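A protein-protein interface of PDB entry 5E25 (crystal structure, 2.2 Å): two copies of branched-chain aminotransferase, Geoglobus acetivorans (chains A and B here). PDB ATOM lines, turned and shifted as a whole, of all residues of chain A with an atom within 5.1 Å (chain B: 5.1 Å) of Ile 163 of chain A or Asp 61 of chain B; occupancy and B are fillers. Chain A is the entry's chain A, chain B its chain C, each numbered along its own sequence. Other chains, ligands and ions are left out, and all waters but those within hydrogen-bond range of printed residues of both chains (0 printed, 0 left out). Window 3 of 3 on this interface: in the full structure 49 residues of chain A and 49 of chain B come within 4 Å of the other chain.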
ATOM      1  N   ILE A 159     -20.087  -9.233  22.833  1.00  0.00           N
ATOM      2  CA  ILE A 159     -18.988  -8.758  23.701  1.00  0.00           C
ATOM      3  C   ILE A 159     -19.414  -8.664  25.161  1.00  0.00           C
ATOM      4  O   ILE A 159     -18.708  -9.119  26.067  1.00  0.00           O
ATOM      5  CB  ILE A 159     -18.395  -7.442  23.165  1.00  0.00           C
ATOM      6  CG1 ILE A 159     -17.594  -7.719  21.861  1.00  0.00           C
ATOM      7  CG2 ILE A 159     -17.465  -6.768  24.209  1.00  0.00           C
ATOM      8  CD1 ILE A 159     -17.412  -6.473  21.010  1.00  0.00           C
ATOM      9  N   LEU A 160     -20.584  -8.092  25.423  1.00  0.00           N
ATOM     10  CA  LEU A 160     -21.073  -8.119  26.821  1.00  0.00           C
ATOM     11  C   LEU A 160     -21.070  -9.515  27.404  1.00  0.00           C
ATOM     12  O   LEU A 160     -20.629  -9.718  28.562  1.00  0.00           O
ATOM     13  CB  LEU A 160     -22.441  -7.481  26.940  1.00  0.00           C
ATOM     14  CG  LEU A 160     -22.347  -5.993  26.700  1.00  0.00           C
ATOM     15  CD1 LEU A 160     -23.757  -5.470  26.477  1.00  0.00           C
ATOM     16  CD2 LEU A 160     -21.644  -5.287  27.887  1.00  0.00           C
ATOM     17  N   ALA A 161     -21.543 -10.482  26.615  1.00  0.00           N
ATOM     18  CA  ALA A 161     -21.528 -11.880  27.034  1.00  0.00           C
ATOM     19  C   ALA A 161     -20.106 -12.373  27.326  1.00  0.00           C
ATOM     20  O   ALA A 161     -19.856 -13.004  28.350  1.00  0.00           O
ATOM     21  CB  ALA A 161     -22.216 -12.791  26.013  1.00  0.00           C
ATOM     22  N   LYS A 162     -19.160 -12.017  26.475  1.00  0.00           N
ATOM     23  CA  LYS A 162     -17.792 -12.493  26.619  1.00  0.00           C
ATOM     24  C   LYS A 162     -17.145 -11.925  27.916  1.00  0.00           C
ATOM     25  O   LYS A 162     -16.463 -12.634  28.633  1.00  0.00           O
ATOM     26  CB  LYS A 162     -17.003 -12.095  25.349  1.00  0.00           C
ATOM     27  CG  LYS A 162     -15.528 -12.498  25.341  1.00  0.00           C
ATOM     28  CD  LYS A 162     -15.305 -14.006  25.533  1.00  0.00           C
ATOM     29  CE  LYS A 162     -13.810 -14.356  25.297  1.00  0.00           C
ATOM     30  NZ  LYS A 162     -13.552 -15.803  25.532  1.00  0.00           N
ATOM     31  N   ILE A 163     -17.442 -10.665  28.206  1.00  0.00           N
ATOM     32  CA  ILE A 163     -17.055  -9.959  29.445  1.00  0.00           C
ATOM     33  C   ILE A 163     -17.572 -10.666  30.654  1.00  0.00           C
ATOM     34  O   ILE A 163     -16.833 -10.792  31.603  1.00  0.00           O
ATOM     35  CB  ILE A 163     -17.582  -8.501  29.474  1.00  0.00           C
ATOM     36  CG1 ILE A 163     -16.861  -7.700  28.359  1.00  0.00           C
ATOM     37  CG2 ILE A 163     -17.435  -7.883  30.891  1.00  0.00           C
ATOM     38  CD1 ILE A 163     -17.436  -6.321  28.082  1.00  0.00           C
ATOM     39  N   GLU A 164     -18.817 -11.157  30.612  1.00  0.00           N
ATOM     40  CA  GLU A 164     -19.336 -11.883  31.748  1.00  0.00           C
ATOM     41  C   GLU A 164     -18.538 -13.164  31.954  1.00  0.00           C
ATOM     42  O   GLU A 164     -18.179 -13.464  33.076  1.00  0.00           O
ATOM     43  CB  GLU A 164     -20.800 -12.283  31.591  1.00  0.00           C
ATOM     44  CG  GLU A 164     -21.812 -11.255  32.016  1.00  0.00           C
ATOM     45  CD  GLU A 164     -23.239 -11.843  31.973  1.00  0.00           C
ATOM     46  OE1 GLU A 164     -23.521 -12.903  32.637  1.00  0.00           O
ATOM     47  OE2 GLU A 164     -24.095 -11.225  31.296  1.00  0.00           O
ATOM     48  N   ALA A 165     -18.309 -13.930  30.882  1.00  0.00           N
ATOM     49  CA  ALA A 165     -17.581 -15.203  31.003  1.00  0.00           C
ATOM     50  C   ALA A 165     -16.138 -14.935  31.443  1.00  0.00           C
ATOM     51  O   ALA A 165     -15.626 -15.679  32.263  1.00  0.00           O
ATOM     52  CB  ALA A 165     -17.636 -16.005  29.710  1.00  0.00           C
ATOM     53  N   ASN A 166     -15.513 -13.848  30.968  1.00  0.00           N
ATOM     54  CA  ASN A 166     -14.187 -13.476  31.494  1.00  0.00           C
ATOM     55  C   ASN A 166     -14.203 -13.354  33.000  1.00  0.00           C
ATOM     56  O   ASN A 166     -13.347 -13.944  33.637  1.00  0.00           O
ATOM     57  CB  ASN A 166     -13.610 -12.203  30.890  1.00  0.00           C
ATOM     58  CG  ASN A 166     -13.355 -12.315  29.394  1.00  0.00           C
ATOM     59  OD1 ASN A 166     -13.196 -11.286  28.724  1.00  0.00           O
ATOM     60  ND2 ASN A 166     -13.315 -13.529  28.863  1.00  0.00           N
ATOM     61  N   ALA A 167     -15.210 -12.662  33.566  1.00  0.00           N
ATOM     62  CA  ALA A 167     -15.228 -12.396  35.000  1.00  0.00           C
ATOM     63  C   ALA A 167     -15.713 -13.602  35.734  1.00  0.00           C
ATOM     64  O   ALA A 167     -15.556 -13.648  36.948  1.00  0.00           O
ATOM     65  CB  ALA A 167     -16.149 -11.231  35.333  1.00  0.00           C
ATOM     66  N   ALA B  57     -19.638   3.986  29.001  1.00  0.00           N
ATOM     67  CA  ALA B  57     -18.355   3.262  28.954  1.00  0.00           C
ATOM     68  C   ALA B  57     -18.291   2.281  30.128  1.00  0.00           C
ATOM     69  O   ALA B  57     -17.904   1.131  29.975  1.00  0.00           O
ATOM     70  CB  ALA B  57     -17.194   4.236  28.959  1.00  0.00           C
ATOM     71  N   ARG B  58     -18.677   2.733  31.315  1.00  0.00           N
ATOM     72  CA  ARG B  58     -18.626   1.839  32.464  1.00  0.00           C
ATOM     73  C   ARG B  58     -19.509   0.560  32.255  1.00  0.00           C
ATOM     74  O   ARG B  58     -19.124  -0.627  32.587  1.00  0.00           O
ATOM     75  CB  ARG B  58     -19.046   2.622  33.725  1.00  0.00           C
ATOM     76  CG  ARG B  58     -18.538   1.949  34.992  1.00  0.00           C
ATOM     77  CD  ARG B  58     -18.884   2.680  36.262  1.00  0.00           C
ATOM     78  NE  ARG B  58     -18.166   2.045  37.372  1.00  0.00           N
ATOM     79  CZ  ARG B  58     -17.052   2.521  37.932  1.00  0.00           C
ATOM     80  NH1 ARG B  58     -16.516   3.658  37.508  1.00  0.00           N
ATOM     81  NH2 ARG B  58     -16.470   1.859  38.935  1.00  0.00           N
ATOM     82  N   VAL B  59     -20.684   0.788  31.666  1.00  0.00           N
ATOM     83  CA  VAL B  59     -21.638  -0.323  31.448  1.00  0.00           C
ATOM     84  C   VAL B  59     -21.013  -1.333  30.503  1.00  0.00           C
ATOM     85  O   VAL B  59     -21.175  -2.556  30.708  1.00  0.00           O
ATOM     86  CB  VAL B  59     -23.022   0.186  30.963  1.00  0.00           C
ATOM     87  CG1 VAL B  59     -23.870  -1.005  30.568  1.00  0.00           C
ATOM     88  CG2 VAL B  59     -23.700   0.976  32.120  1.00  0.00           C
ATOM     89  N   ILE B  60     -20.258  -0.832  29.510  1.00  0.00           N
ATOM     90  CA  ILE B  60     -19.511  -1.747  28.610  1.00  0.00           C
ATOM     91  C   ILE B  60     -18.090  -2.111  29.099  1.00  0.00           C
ATOM     92  O   ILE B  60     -17.261  -2.756  28.351  1.00  0.00           O
ATOM     93  CB  ILE B  60     -19.499  -1.305  27.102  1.00  0.00           C
ATOM     94  CG1 ILE B  60     -18.624  -0.060  26.841  1.00  0.00           C
ATOM     95  CG2 ILE B  60     -20.911  -1.165  26.581  1.00  0.00           C
ATOM     96  CD1 ILE B  60     -18.380   0.216  25.339  1.00  0.00           C
ATOM     97  N   ASP B  61     -17.818  -1.762  30.353  1.00  0.00           N
ATOM     98  CA  ASP B  61     -16.500  -2.115  30.968  1.00  0.00           C
ATOM     99  C   ASP B  61     -15.315  -1.559  30.176  1.00  0.00           C
ATOM    100  O   ASP B  61     -14.358  -2.277  29.891  1.00  0.00           O
ATOM    101  CB  ASP B  61     -16.356  -3.641  31.082  1.00  0.00           C
ATOM    102  CG  ASP B  61     -15.388  -4.047  32.167  1.00  0.00           C
ATOM    103  OD1 ASP B  61     -15.180  -3.314  33.131  1.00  0.00           O
ATOM    104  OD2 ASP B  61     -14.833  -5.119  32.084  1.00  0.00           O
ATOM    105  N   LEU B  62     -15.437  -0.310  29.735  1.00  0.00           N
ATOM    106  CA  LEU B  62     -14.365   0.312  28.964  1.00  0.00           C
ATOM    107  C   LEU B  62     -13.786   1.445  29.781  1.00  0.00           C
ATOM    108  O   LEU B  62     -14.542   2.310  30.230  1.00  0.00           O
ATOM    109  CB  LEU B  62     -14.954   0.879  27.658  1.00  0.00           C
ATOM    110  CG  LEU B  62     -14.089   1.740  26.733  1.00  0.00           C
ATOM    111  CD1 LEU B  62     -12.823   1.005  26.292  1.00  0.00           C
ATOM    112  CD2 LEU B  62     -14.928   2.169  25.542  1.00  0.00           C
ATOM    113  N   LYS B  63     -12.470   1.478  29.974  1.00  0.00           N
ATOM    114  CA  LYS B  63     -11.882   2.644  30.693  1.00  0.00           C
ATOM    115  C   LYS B  63     -11.573   3.799  29.733  1.00  0.00           C
ATOM    116  O   LYS B  63     -10.750   3.674  28.874  1.00  0.00           O
ATOM    117  CB  LYS B  63     -10.638   2.249  31.515  1.00  0.00           C
ATOM    118  CG  LYS B  63     -10.908   1.912  32.979  1.00  0.00           C
ATOM    119  N   ARG B  95     -12.994   0.671  21.999  1.00  0.00           N
ATOM    120  CA  ARG B  95     -12.128  -0.328  22.652  1.00  0.00           C
ATOM    121  C   ARG B  95     -10.641  -0.269  22.191  1.00  0.00           C
ATOM    122  O   ARG B  95      -9.767  -0.701  22.925  1.00  0.00           O
ATOM    123  CB  ARG B  95     -12.706  -1.743  22.377  1.00  0.00           C
ATOM    124  CG  ARG B  95     -12.098  -2.880  23.192  1.00  0.00           C
ATOM    125  CD  ARG B  95     -12.561  -2.786  24.639  1.00  0.00           C
ATOM    126  NE  ARG B  95     -14.011  -2.990  24.660  1.00  0.00           N
ATOM    127  CZ  ARG B  95     -14.756  -3.057  25.766  1.00  0.00           C
ATOM    128  NH1 ARG B  95     -14.171  -2.925  26.934  1.00  0.00           N
ATOM    129  NH2 ARG B  95     -16.081  -3.283  25.696  1.00  0.00           N
ATOM    130  N   PRO B 104     -12.432  -8.414  24.713  1.00  0.00           N
ATOM    131  CA  PRO B 104     -11.911  -7.059  24.950  1.00  0.00           C
ATOM    132  C   PRO B 104     -10.590  -7.031  25.765  1.00  0.00           C
ATOM    133  O   PRO B 104      -9.834  -6.059  25.675  1.00  0.00           O
ATOM    134  CB  PRO B 104     -13.040  -6.381  25.729  1.00  0.00           C
ATOM    135  CG  PRO B 104     -13.743  -7.513  26.409  1.00  0.00           C
ATOM    136  CD  PRO B 104     -13.722  -8.637  25.404  1.00  0.00           C
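No position is printed for both chains. Of the 4 pairs that touch across the chains among the printed residues, none has its exchanged pair printed and touching as well.
The backbone carbonyl oxygen (O) of Ile 60 of chain B is in hydrogen-bond range of the guanidinium group (NH2) of Arg 95 of chain B (3.0 Å). The guanidinium group of Arg 95 of chain B is in hydrogen-bond range of the backbone carbonyl oxygen of Asp 61 of chain B.
Along chain A the printed residues that touch a printed residue of chain B span positions 160 to 163. Of the 9 printed residues of chain B, 4 touch a printed residue of chain A. Hydrophobic or aromatic side chains of chain B that line the printed part of chain A: Pro 104.
Printed residues of chain B within 4 Å of Leu 160 of chain A: Val 59. Ile 163 of chain A touches just these residues of chain B: Ile 60, Asp 61 and Pro 104. Glu 164 of chain A touches none of the printed residues of chain B. Of the printed residues of chain A, Val 59 of chain B touches Leu 160. Of the printed residues of chain A, Ile 60 of chain B touches Ile 163. Of chain A, only Ile 163 comes within 4 Å of Asp 61 of chain B. Of the printed residues of chain A, Pro 104 of chain B touches Ile 163 (3.7 Å). The nearest residue of chain B that does not touch Ile 163 of chain A is Arg 95 of chain B (4.1 Å). The nearest printed residue of chain A that does not touch Asp 61 of chain B is Leu 160 of chain A (5.8 Å). The nearest printed residue of chain A that does not touch Pro 104 of chain B is Lys 162 of chain A (4.3 Å).
Among the printed residues, merely in contact across the chains: Leu 160 of chain A with Val 59 of chain B (3.95 Å), Ile 163 of chain A with Ile 60 of chain B (3.6 Å), Ile 163 of chain A with Asp 61 of chain B (3.98 Å) and Ile 163 of chain A with Pro 104 of chain B (3.7 Å).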
